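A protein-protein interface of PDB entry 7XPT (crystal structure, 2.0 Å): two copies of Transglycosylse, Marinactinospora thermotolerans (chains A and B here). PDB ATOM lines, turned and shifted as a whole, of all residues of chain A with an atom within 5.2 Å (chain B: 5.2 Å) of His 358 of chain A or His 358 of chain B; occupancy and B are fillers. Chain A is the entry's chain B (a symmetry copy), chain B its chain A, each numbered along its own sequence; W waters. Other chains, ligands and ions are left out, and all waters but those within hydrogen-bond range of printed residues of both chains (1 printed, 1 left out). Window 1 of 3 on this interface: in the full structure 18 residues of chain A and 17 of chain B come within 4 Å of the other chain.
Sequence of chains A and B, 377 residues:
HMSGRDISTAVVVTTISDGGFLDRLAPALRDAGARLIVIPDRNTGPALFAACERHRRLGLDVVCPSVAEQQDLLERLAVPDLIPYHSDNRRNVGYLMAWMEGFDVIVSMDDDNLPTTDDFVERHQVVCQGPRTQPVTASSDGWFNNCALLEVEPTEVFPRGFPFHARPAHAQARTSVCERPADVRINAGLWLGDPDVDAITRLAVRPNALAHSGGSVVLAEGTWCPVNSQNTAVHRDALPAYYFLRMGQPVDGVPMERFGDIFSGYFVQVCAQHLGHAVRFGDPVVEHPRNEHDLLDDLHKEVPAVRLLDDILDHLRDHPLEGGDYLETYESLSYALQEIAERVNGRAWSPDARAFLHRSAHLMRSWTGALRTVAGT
Of the 12 printed residues of chain A, 7 touch a printed residue of chain B. Hydrophobic or aromatic side chains of chain A that line the printed part of chain B: Ala 355, His 358 and His 362. Of the 12 printed residues of chain B, 7 touch a printed residue of chain A. Hydrophobic or aromatic side chains of chain B within 4 Å of the printed part of chain A: Ala 355, His 358 and His 362. Among the printed residues, 16 pairs touch across the chains.
NE2 of His 358 of chain B is in hydrogen-bond range of OE2 of Glu 342 of chain B, at 2.7 Å. The side-chain amide nitrogen (NE2) of Gln 338 of chain B lies within hydrogen-bond range of a ring nitrogen (ND1) of His 358 of chain B. The side-chain carboxylate (OE2) of Glu 342 of chain A is in hydrogen-bond range of a ring nitrogen (NE2) of His 358 of chain A, 2.7 Å away. NH1 of Arg 354 of chain B sits at hydrogen-bond distance from O of Ala 341 of chain B (2.7 Å). ND1 of His 358 of chain A sits at hydrogen-bond distance from NE2 of Gln 338 of chain A, 3.0 Å away. The guanidinium group (NH1) of Arg 354 of chain A lies within hydrogen-bond range of the backbone carbonyl oxygen (O) of Ala 341 of chain A, 2.8 Å away.
Of the printed residues of chain B, Gln 338 of chain A touches His 362. Of the printed residues of chain B, Arg 354 of chain A touches Arg 359. His 358 of chain A touches just these residues of chain B: His 358 (3.9 Å), Arg 359 (3.5 Å) and His 362 (3.4 Å). Printed residues of chain B within 4 Å of Arg 359 of chain A: Glu 342 (2.7 Å), Arg 354 (3.4 Å), Ala 355 (3.9 Å) and His 358 (3.5 Å). Of the printed residues of chain A, Gln 338 of chain B touches His 362. Ala 341 of chain B touches none of the printed residues of chain A. Of the printed residues of chain A, Ala 355 of chain B touches Ala 355 and Arg 359. Of chain A, only His 358, Arg 359 and His 362 come within 4 Å of His 358 of chain B.
Water W1 bridges ND1 of His 362 of chain A (2.5 Å) and OE1 of Gln 338 of chain B (2.8 Å).
NE of Arg 359 of chain B lies within salt-bridge range of OE2 of Glu 342 of chain A (2.7 Å). OE2 of Glu 342 of chain B lies within salt-bridge range of NE of Arg 359 of chain A (2.7 Å).
Gln 338 of chain A touches His 362 of chain B. CD2 of His 362 of chain B touches CG of Glu 342 of chain A, at 3.9 Å. Arg 359 of chain B touches Ala 355 of chain A. Arg 359 of chain B touches His 358 of chain A. CE1 of His 358 of chain A touches CG of His 362 of chain B (3.4 Å). Arg 359 of chain A touches Ala 355 of chain B (CD to N, 3.9 Å). Arg 359 of chain A touches His 358 of chain B. His 362 of chain A touches Gln 338 of chain B (ND1 to CB, 3.5 Å). NE2 of His 362 of chain A touches CG of Glu 342 of chain B, at 3.95 Å. His 362 of chain A touches His 358 of chain B.
Glu 342 of chain A touches Arg 359 of chain B, and with the chains exchanged Arg 359 of chain A touches Glu 342 of chain B. Glu 342 of chain A touches His 362 of chain B, and with the chains exchanged His 362 of chain A touches Glu 342 of chain B. Ala 355 of chain A touches its own counterpart, Ala 355 of chain B. His 358 of chain A touches its own counterpart, His 358 of chain B. Positions printed for both chains: 338, 341, 342, 354, 355, 356, 357, 358, 359, 360, 361 and 362. Of the 16 pairs that touch across the chains among the printed residues, 16 have their exchanged pair printed and touching as well.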
ATOM      1  N   GLN A 338       5.255  31.628  -6.021  1.00  0.00           N
ATOM      2  CA  GLN A 338       5.953  31.041  -7.159  1.00  0.00           C
ATOM      3  C   GLN A 338       7.404  31.502  -7.220  1.00  0.00           C
ATOM      4  O   GLN A 338       8.289  30.735  -7.618  1.00  0.00           O
ATOM      5  CB  GLN A 338       5.224  31.383  -8.458  1.00  0.00           C
ATOM      6  CG  GLN A 338       3.844  30.771  -8.550  1.00  0.00           C
ATOM      7  CD  GLN A 338       3.306  30.759  -9.963  1.00  0.00           C
ATOM      8  OE1 GLN A 338       2.615  31.689 -10.384  1.00  0.00           O
ATOM      9  NE2 GLN A 338       3.621  29.702 -10.706  1.00  0.00           N
ATOM     10  N   ALA A 341       9.233  29.589  -4.582  1.00  0.00           N
ATOM     11  CA  ALA A 341       9.432  28.182  -4.914  1.00  0.00           C
ATOM     12  C   ALA A 341      10.766  27.939  -5.610  1.00  0.00           C
ATOM     13  O   ALA A 341      11.323  26.839  -5.514  1.00  0.00           O
ATOM     14  CB  ALA A 341       8.281  27.681  -5.789  1.00  0.00           C
ATOM     15  N   GLU A 342      11.299  28.944  -6.307  1.00  0.00           N
ATOM     16  CA  GLU A 342      12.549  28.788  -7.037  1.00  0.00           C
ATOM     17  C   GLU A 342      13.761  29.339  -6.295  1.00  0.00           C
ATOM     18  O   GLU A 342      14.891  28.983  -6.643  1.00  0.00           O
ATOM     19  CB  GLU A 342      12.452  29.464  -8.410  1.00  0.00           C
ATOM     20  CG  GLU A 342      11.304  28.952  -9.277  1.00  0.00           C
ATOM     21  CD  GLU A 342      11.421  27.468  -9.585  1.00  0.00           C
ATOM     22  OE1 GLU A 342      12.547  27.004  -9.861  1.00  0.00           O
ATOM     23  OE2 GLU A 342      10.388  26.767  -9.544  1.00  0.00           O
ATOM     24  N   ARG A 354       9.044  22.066  -4.974  1.00  0.00           N
ATOM     25  CA  ARG A 354       8.930  23.370  -5.617  1.00  0.00           C
ATOM     26  C   ARG A 354       7.657  23.463  -6.451  1.00  0.00           C
ATOM     27  O   ARG A 354       6.991  24.504  -6.470  1.00  0.00           O
ATOM     28  CB  ARG A 354      10.159  23.636  -6.485  1.00  0.00           C
ATOM     29  CG  ARG A 354      11.488  23.530  -5.750  1.00  0.00           C
ATOM     30  CD  ARG A 354      12.637  23.987  -6.635  1.00  0.00           C
ATOM     31  NE  ARG A 354      13.933  23.823  -5.986  1.00  0.00           N
ATOM     32  CZ  ARG A 354      14.486  24.719  -5.177  1.00  0.00           C
ATOM     33  NH1 ARG A 354      13.876  25.856  -4.885  1.00  0.00           N
ATOM     34  NH2 ARG A 354      15.680  24.466  -4.648  1.00  0.00           N
ATOM     35  N   ALA A 355       7.302  22.380  -7.146  1.00  0.00           N
ATOM     36  CA  ALA A 355       6.103  22.383  -7.975  1.00  0.00           C
ATOM     37  C   ALA A 355       4.825  22.415  -7.147  1.00  0.00           C
ATOM     38  O   ALA A 355       3.782  22.835  -7.662  1.00  0.00           O
ATOM     39  CB  ALA A 355       6.103  21.165  -8.900  1.00  0.00           C
ATOM     40  N   PHE A 356       4.881  21.980  -5.884  1.00  0.00           N
ATOM     41  CA  PHE A 356       3.719  22.094  -5.007  1.00  0.00           C
ATOM     42  C   PHE A 356       3.271  23.544  -4.866  1.00  0.00           C
ATOM     43  O   PHE A 356       2.072  23.839  -4.917  1.00  0.00           O
ATOM     44  CB  PHE A 356       4.033  21.494  -3.635  1.00  0.00           C
ATOM     45  CG  PHE A 356       3.278  22.136  -2.501  1.00  0.00           C
ATOM     46  CD1 PHE A 356       1.921  21.908  -2.331  1.00  0.00           C
ATOM     47  CD2 PHE A 356       3.931  22.957  -1.596  1.00  0.00           C
ATOM     48  CE1 PHE A 356       1.229  22.496  -1.287  1.00  0.00           C
ATOM     49  CE2 PHE A 356       3.244  23.546  -0.549  1.00  0.00           C
ATOM     50  CZ  PHE A 356       1.893  23.316  -0.395  1.00  0.00           C
ATOM     51  N   LEU A 357       4.222  24.465  -4.685  1.00  0.00           N
ATOM     52  CA  LEU A 357       3.859  25.872  -4.550  1.00  0.00           C
ATOM     53  C   LEU A 357       3.336  26.449  -5.859  1.00  0.00           C
ATOM     54  O   LEU A 357       2.526  27.383  -5.845  1.00  0.00           O
ATOM     55  CB  LEU A 357       5.057  26.680  -4.053  1.00  0.00           C
ATOM     56  CG  LEU A 357       5.420  26.495  -2.576  1.00  0.00           C
ATOM     57  CD1 LEU A 357       6.753  27.157  -2.252  1.00  0.00           C
ATOM     58  CD2 LEU A 357       4.317  27.049  -1.692  1.00  0.00           C
ATOM     59  N   HIS A 358       3.778  25.910  -6.998  1.00  0.00           N
ATOM     60  CA  HIS A 358       3.313  26.436  -8.277  1.00  0.00           C
ATOM     61  C   HIS A 358       1.877  26.014  -8.562  1.00  0.00           C
ATOM     62  O   HIS A 358       1.066  26.828  -9.019  1.00  0.00           O
ATOM     63  CB  HIS A 358       4.244  25.986  -9.403  1.00  0.00           C
ATOM     64  CG  HIS A 358       5.601  26.616  -9.351  1.00  0.00           C
ATOM     65  ND1 HIS A 358       5.803  27.965  -9.545  1.00  0.00           N
ATOM     66  CD2 HIS A 358       6.825  26.082  -9.126  1.00  0.00           C
ATOM     67  CE1 HIS A 358       7.092  28.234  -9.445  1.00  0.00           C
ATOM     68  NE2 HIS A 358       7.735  27.109  -9.193  1.00  0.00           N
ATOM     69  N   ARG A 359       1.541  24.748  -8.302  1.00  0.00           N
ATOM     70  CA  ARG A 359       0.161  24.313  -8.493  1.00  0.00           C
ATOM     71  C   ARG A 359      -0.763  24.918  -7.443  1.00  0.00           C
ATOM     72  O   ARG A 359      -1.924  25.219  -7.743  1.00  0.00           O
ATOM     73  CB  ARG A 359       0.069  22.787  -8.469  1.00  0.00           C
ATOM     74  CG  ARG A 359      -1.350  22.256  -8.644  1.00  0.00           C
ATOM     75  CD  ARG A 359      -1.367  20.803  -9.095  1.00  0.00           C
ATOM     76  NE  ARG A 359      -2.710  20.360  -9.459  1.00  0.00           N
ATOM     77  CZ  ARG A 359      -3.430  19.486  -8.768  1.00  0.00           C
ATOM     78  NH1 ARG A 359      -2.959  18.915  -7.670  1.00  0.00           N
ATOM     79  NH2 ARG A 359      -4.650  19.171  -9.193  1.00  0.00           N
ATOM     80  N   SER A 360      -0.268  25.103  -6.215  1.00  0.00           N
ATOM     81  CA  SER A 360      -1.062  25.779  -5.197  1.00  0.00           C
ATOM     82  C   SER A 360      -1.396  27.204  -5.619  1.00  0.00           C
ATOM     83  O   SER A 360      -2.523  27.670  -5.421  1.00  0.00           O
ATOM     84  CB  SER A 360      -0.317  25.783  -3.861  1.00  0.00           C
ATOM     85  OG  SER A 360      -0.136  24.468  -3.364  1.00  0.00           O
ATOM     86  N   ALA A 361      -0.426  27.902  -6.214  1.00  0.00           N
ATOM     87  CA  ALA A 361      -0.646  29.283  -6.629  1.00  0.00           C
ATOM     88  C   ALA A 361      -1.678  29.368  -7.746  1.00  0.00           C
ATOM     89  O   ALA A 361      -2.463  30.322  -7.800  1.00  0.00           O
ATOM     90  CB  ALA A 361       0.675  29.911  -7.066  1.00  0.00           C
ATOM     91  N   HIS A 362      -1.691  28.386  -8.648  1.00  0.00           N
ATOM     92  CA  HIS A 362      -2.705  28.360  -9.696  1.00  0.00           C
ATOM     93  C   HIS A 362      -4.093  28.146  -9.104  1.00  0.00           C
ATOM     94  O   HIS A 362      -5.050  28.835  -9.477  1.00  0.00           O
ATOM     95  CB  HIS A 362      -2.382  27.271 -10.717  1.00  0.00           C
ATOM     96  CG  HIS A 362      -3.450  27.077 -11.750  1.00  0.00           C
ATOM     97  ND1 HIS A 362      -3.461  27.763 -12.945  1.00  0.00           N
ATOM     98  CD2 HIS A 362      -4.545  26.282 -11.762  1.00  0.00           C
ATOM     99  CE1 HIS A 362      -4.516  27.395 -13.651  1.00  0.00           C
ATOM    100  NE2 HIS A 362      -5.189  26.497 -12.956  1.00  0.00           N
ATOM    101  N   GLN B 338      -1.338  25.487 -17.870  1.00  0.00           N
ATOM    102  CA  GLN B 338      -1.840  25.397 -16.503  1.00  0.00           C
ATOM    103  C   GLN B 338      -3.315  25.012 -16.476  1.00  0.00           C
ATOM    104  O   GLN B 338      -3.752  24.274 -15.584  1.00  0.00           O
ATOM    105  CB  GLN B 338      -1.613  26.719 -15.775  1.00  0.00           C
ATOM    106  CG  GLN B 338      -0.147  27.082 -15.645  1.00  0.00           C
ATOM    107  CD  GLN B 338       0.087  28.226 -14.685  1.00  0.00           C
ATOM    108  OE1 GLN B 338       0.073  29.393 -15.078  1.00  0.00           O
ATOM    109  NE2 GLN B 338       0.303  27.897 -13.415  1.00  0.00           N
ATOM    110  N   ALA B 341      -3.441  21.339 -17.198  1.00  0.00           N
ATOM    111  CA  ALA B 341      -2.985  20.525 -16.075  1.00  0.00           C
ATOM    112  C   ALA B 341      -4.133  20.113 -15.163  1.00  0.00           C
ATOM    113  O   ALA B 341      -4.070  19.051 -14.531  1.00  0.00           O
ATOM    114  CB  ALA B 341      -1.922  21.283 -15.280  1.00  0.00           C
ATOM    115  N   GLU B 342      -5.186  20.926 -15.077  1.00  0.00           N
ATOM    116  CA  GLU B 342      -6.309  20.619 -14.203  1.00  0.00           C
ATOM    117  C   GLU B 342      -7.481  19.970 -14.925  1.00  0.00           C
ATOM    118  O   GLU B 342      -8.351  19.396 -14.261  1.00  0.00           O
ATOM    119  CB  GLU B 342      -6.796  21.891 -13.495  1.00  0.00           C
ATOM    120  CG  GLU B 342      -5.721  22.591 -12.679  1.00  0.00           C
ATOM    121  CD  GLU B 342      -5.158  21.716 -11.576  1.00  0.00           C
ATOM    122  OE1 GLU B 342      -5.943  20.998 -10.922  1.00  0.00           O
ATOM    123  OE2 GLU B 342      -3.928  21.742 -11.368  1.00  0.00           O
ATOM    124  N   ARG B 354       0.551  16.767 -12.573  1.00  0.00           N
ATOM    125  CA  ARG B 354      -0.120  18.031 -12.854  1.00  0.00           C
ATOM    126  C   ARG B 354       0.752  19.214 -12.456  1.00  0.00           C
ATOM    127  O   ARG B 354       0.831  20.209 -13.187  1.00  0.00           O
ATOM    128  CB  ARG B 354      -1.463  18.083 -12.128  1.00  0.00           C
ATOM    129  CG  ARG B 354      -2.393  16.924 -12.454  1.00  0.00           C
ATOM    130  CD  ARG B 354      -3.713  17.061 -11.716  1.00  0.00           C
ATOM    131  NE  ARG B 354      -4.625  15.962 -12.009  1.00  0.00           N
ATOM    132  CZ  ARG B 354      -5.501  15.960 -13.003  1.00  0.00           C
ATOM    133  NH1 ARG B 354      -5.607  16.987 -13.831  1.00  0.00           N
ATOM    134  NH2 ARG B 354      -6.292  14.903 -13.171  1.00  0.00           N
ATOM    135  N   ALA B 355       1.418  19.124 -11.302  1.00  0.00           N
ATOM    136  CA  ALA B 355       2.299  20.197 -10.860  1.00  0.00           C
ATOM    137  C   ALA B 355       3.506  20.367 -11.771  1.00  0.00           C
ATOM    138  O   ALA B 355       4.130  21.434 -11.756  1.00  0.00           O
ATOM    139  CB  ALA B 355       2.754  19.940  -9.423  1.00  0.00           C
ATOM    140  N   PHE B 356       3.851  19.343 -12.556  1.00  0.00           N
ATOM    141  CA  PHE B 356       4.928  19.488 -13.532  1.00  0.00           C
ATOM    142  C   PHE B 356       4.607  20.576 -14.550  1.00  0.00           C
ATOM    143  O   PHE B 356       5.471  21.392 -14.893  1.00  0.00           O
ATOM    144  CB  PHE B 356       5.182  18.150 -14.229  1.00  0.00           C
ATOM    145  CG  PHE B 356       5.666  18.282 -15.646  1.00  0.00           C
ATOM    146  CD1 PHE B 356       6.959  18.701 -15.919  1.00  0.00           C
ATOM    147  CD2 PHE B 356       4.831  17.971 -16.708  1.00  0.00           C
ATOM    148  CE1 PHE B 356       7.405  18.822 -17.223  1.00  0.00           C
ATOM    149  CE2 PHE B 356       5.272  18.087 -18.015  1.00  0.00           C
ATOM    150  CZ  PHE B 356       6.560  18.512 -18.271  1.00  0.00           C
ATOM    151  N   LEU B 357       3.368  20.605 -15.046  1.00  0.00           N
ATOM    152  CA  LEU B 357       2.985  21.641 -16.000  1.00  0.00           C
ATOM    153  C   LEU B 357       2.930  23.014 -15.346  1.00  0.00           C
ATOM    154  O   LEU B 357       3.206  24.023 -16.005  1.00  0.00           O
ATOM    155  CB  LEU B 357       1.637  21.298 -16.634  1.00  0.00           C
ATOM    156  CG  LEU B 357       1.627  20.099 -17.586  1.00  0.00           C
ATOM    157  CD1 LEU B 357       0.203  19.704 -17.962  1.00  0.00           C
ATOM    158  CD2 LEU B 357       2.447  20.405 -18.833  1.00  0.00           C
ATOM    159  N   HIS B 358       2.580  23.076 -14.059  1.00  0.00           N
ATOM    160  CA  HIS B 358       2.489  24.369 -13.389  1.00  0.00           C
ATOM    161  C   HIS B 358       3.868  24.972 -13.148  1.00  0.00           C
ATOM    162  O   HIS B 358       4.064  26.178 -13.343  1.00  0.00           O
ATOM    163  CB  HIS B 358       1.720  24.228 -12.075  1.00  0.00           C
ATOM    164  CG  HIS B 358       0.262  23.945 -12.259  1.00  0.00           C
ATOM    165  ND1 HIS B 358      -0.604  24.852 -12.831  1.00  0.00           N
ATOM    166  CD2 HIS B 358      -0.481  22.856 -11.952  1.00  0.00           C
ATOM    167  CE1 HIS B 358      -1.820  24.336 -12.863  1.00  0.00           C
ATOM    168  NE2 HIS B 358      -1.773  23.126 -12.335  1.00  0.00           N
ATOM    169  N   ARG B 359       4.836  24.159 -12.718  1.00  0.00           N
ATOM    170  CA  ARG B 359       6.189  24.679 -12.542  1.00  0.00           C
ATOM    171  C   ARG B 359       6.834  24.987 -13.887  1.00  0.00           C
ATOM    172  O   ARG B 359       7.568  25.973 -14.018  1.00  0.00           O
ATOM    173  CB  ARG B 359       7.048  23.695 -11.743  1.00  0.00           C
ATOM    174  CG  ARG B 359       8.501  24.148 -11.592  1.00  0.00           C
ATOM    175  CD  ARG B 359       9.199  23.507 -10.397  1.00  0.00           C
ATOM    176  NE  ARG B 359      10.517  24.093 -10.165  1.00  0.00           N
ATOM    177  CZ  ARG B 359      11.663  23.428 -10.212  1.00  0.00           C
ATOM    178  NH1 ARG B 359      11.701  22.123 -10.438  1.00  0.00           N
ATOM    179  NH2 ARG B 359      12.803  24.086 -10.018  1.00  0.00           N
ATOM    180  N   SER B 360       6.563  24.161 -14.900  1.00  0.00           N
ATOM    181  CA  SER B 360       7.084  24.435 -16.235  1.00  0.00           C
ATOM    182  C   SER B 360       6.573  25.771 -16.764  1.00  0.00           C
ATOM    183  O   SER B 360       7.331  26.536 -17.369  1.00  0.00           O
ATOM    184  CB  SER B 360       6.707  23.302 -17.190  1.00  0.00           C
ATOM    185  OG  SER B 360       7.309  22.078 -16.798  1.00  0.00           O
ATOM    186  N   ALA B 361       5.292  26.072 -16.533  1.00  0.00           N
ATOM    187  CA  ALA B 361       4.727  27.326 -17.023  1.00  0.00           C
ATOM    188  C   ALA B 361       5.395  28.529 -16.369  1.00  0.00           C
ATOM    189  O   ALA B 361       5.694  29.525 -17.041  1.00  0.00           O
ATOM    190  CB  ALA B 361       3.218  27.352 -16.784  1.00  0.00           C
ATOM    191  N   HIS B 362       5.634  28.459 -15.058  1.00  0.00           N
ATOM    192  CA  HIS B 362       6.365  29.528 -14.384  1.00  0.00           C
ATOM    193  C   HIS B 362       7.766  29.690 -14.965  1.00  0.00           C
ATOM    194  O   HIS B 362       8.226  30.815 -15.192  1.00  0.00           O
ATOM    195  CB  HIS B 362       6.440  29.251 -12.883  1.00  0.00           C
ATOM    196  CG  HIS B 362       7.271  30.241 -12.126  1.00  0.00           C
ATOM    197  ND1 HIS B 362       6.762  31.430 -11.648  1.00  0.00           N
ATOM    198  CD2 HIS B 362       8.576  30.219 -11.764  1.00  0.00           C
ATOM    199  CE1 HIS B 362       7.717  32.096 -11.023  1.00  0.00           C
ATOM    200  NE2 HIS B 362       8.828  31.383 -11.079  1.00  0.00           N
HETATM  201  O   HOH W   1      -2.187  29.815 -13.403  1.00  0.00           O
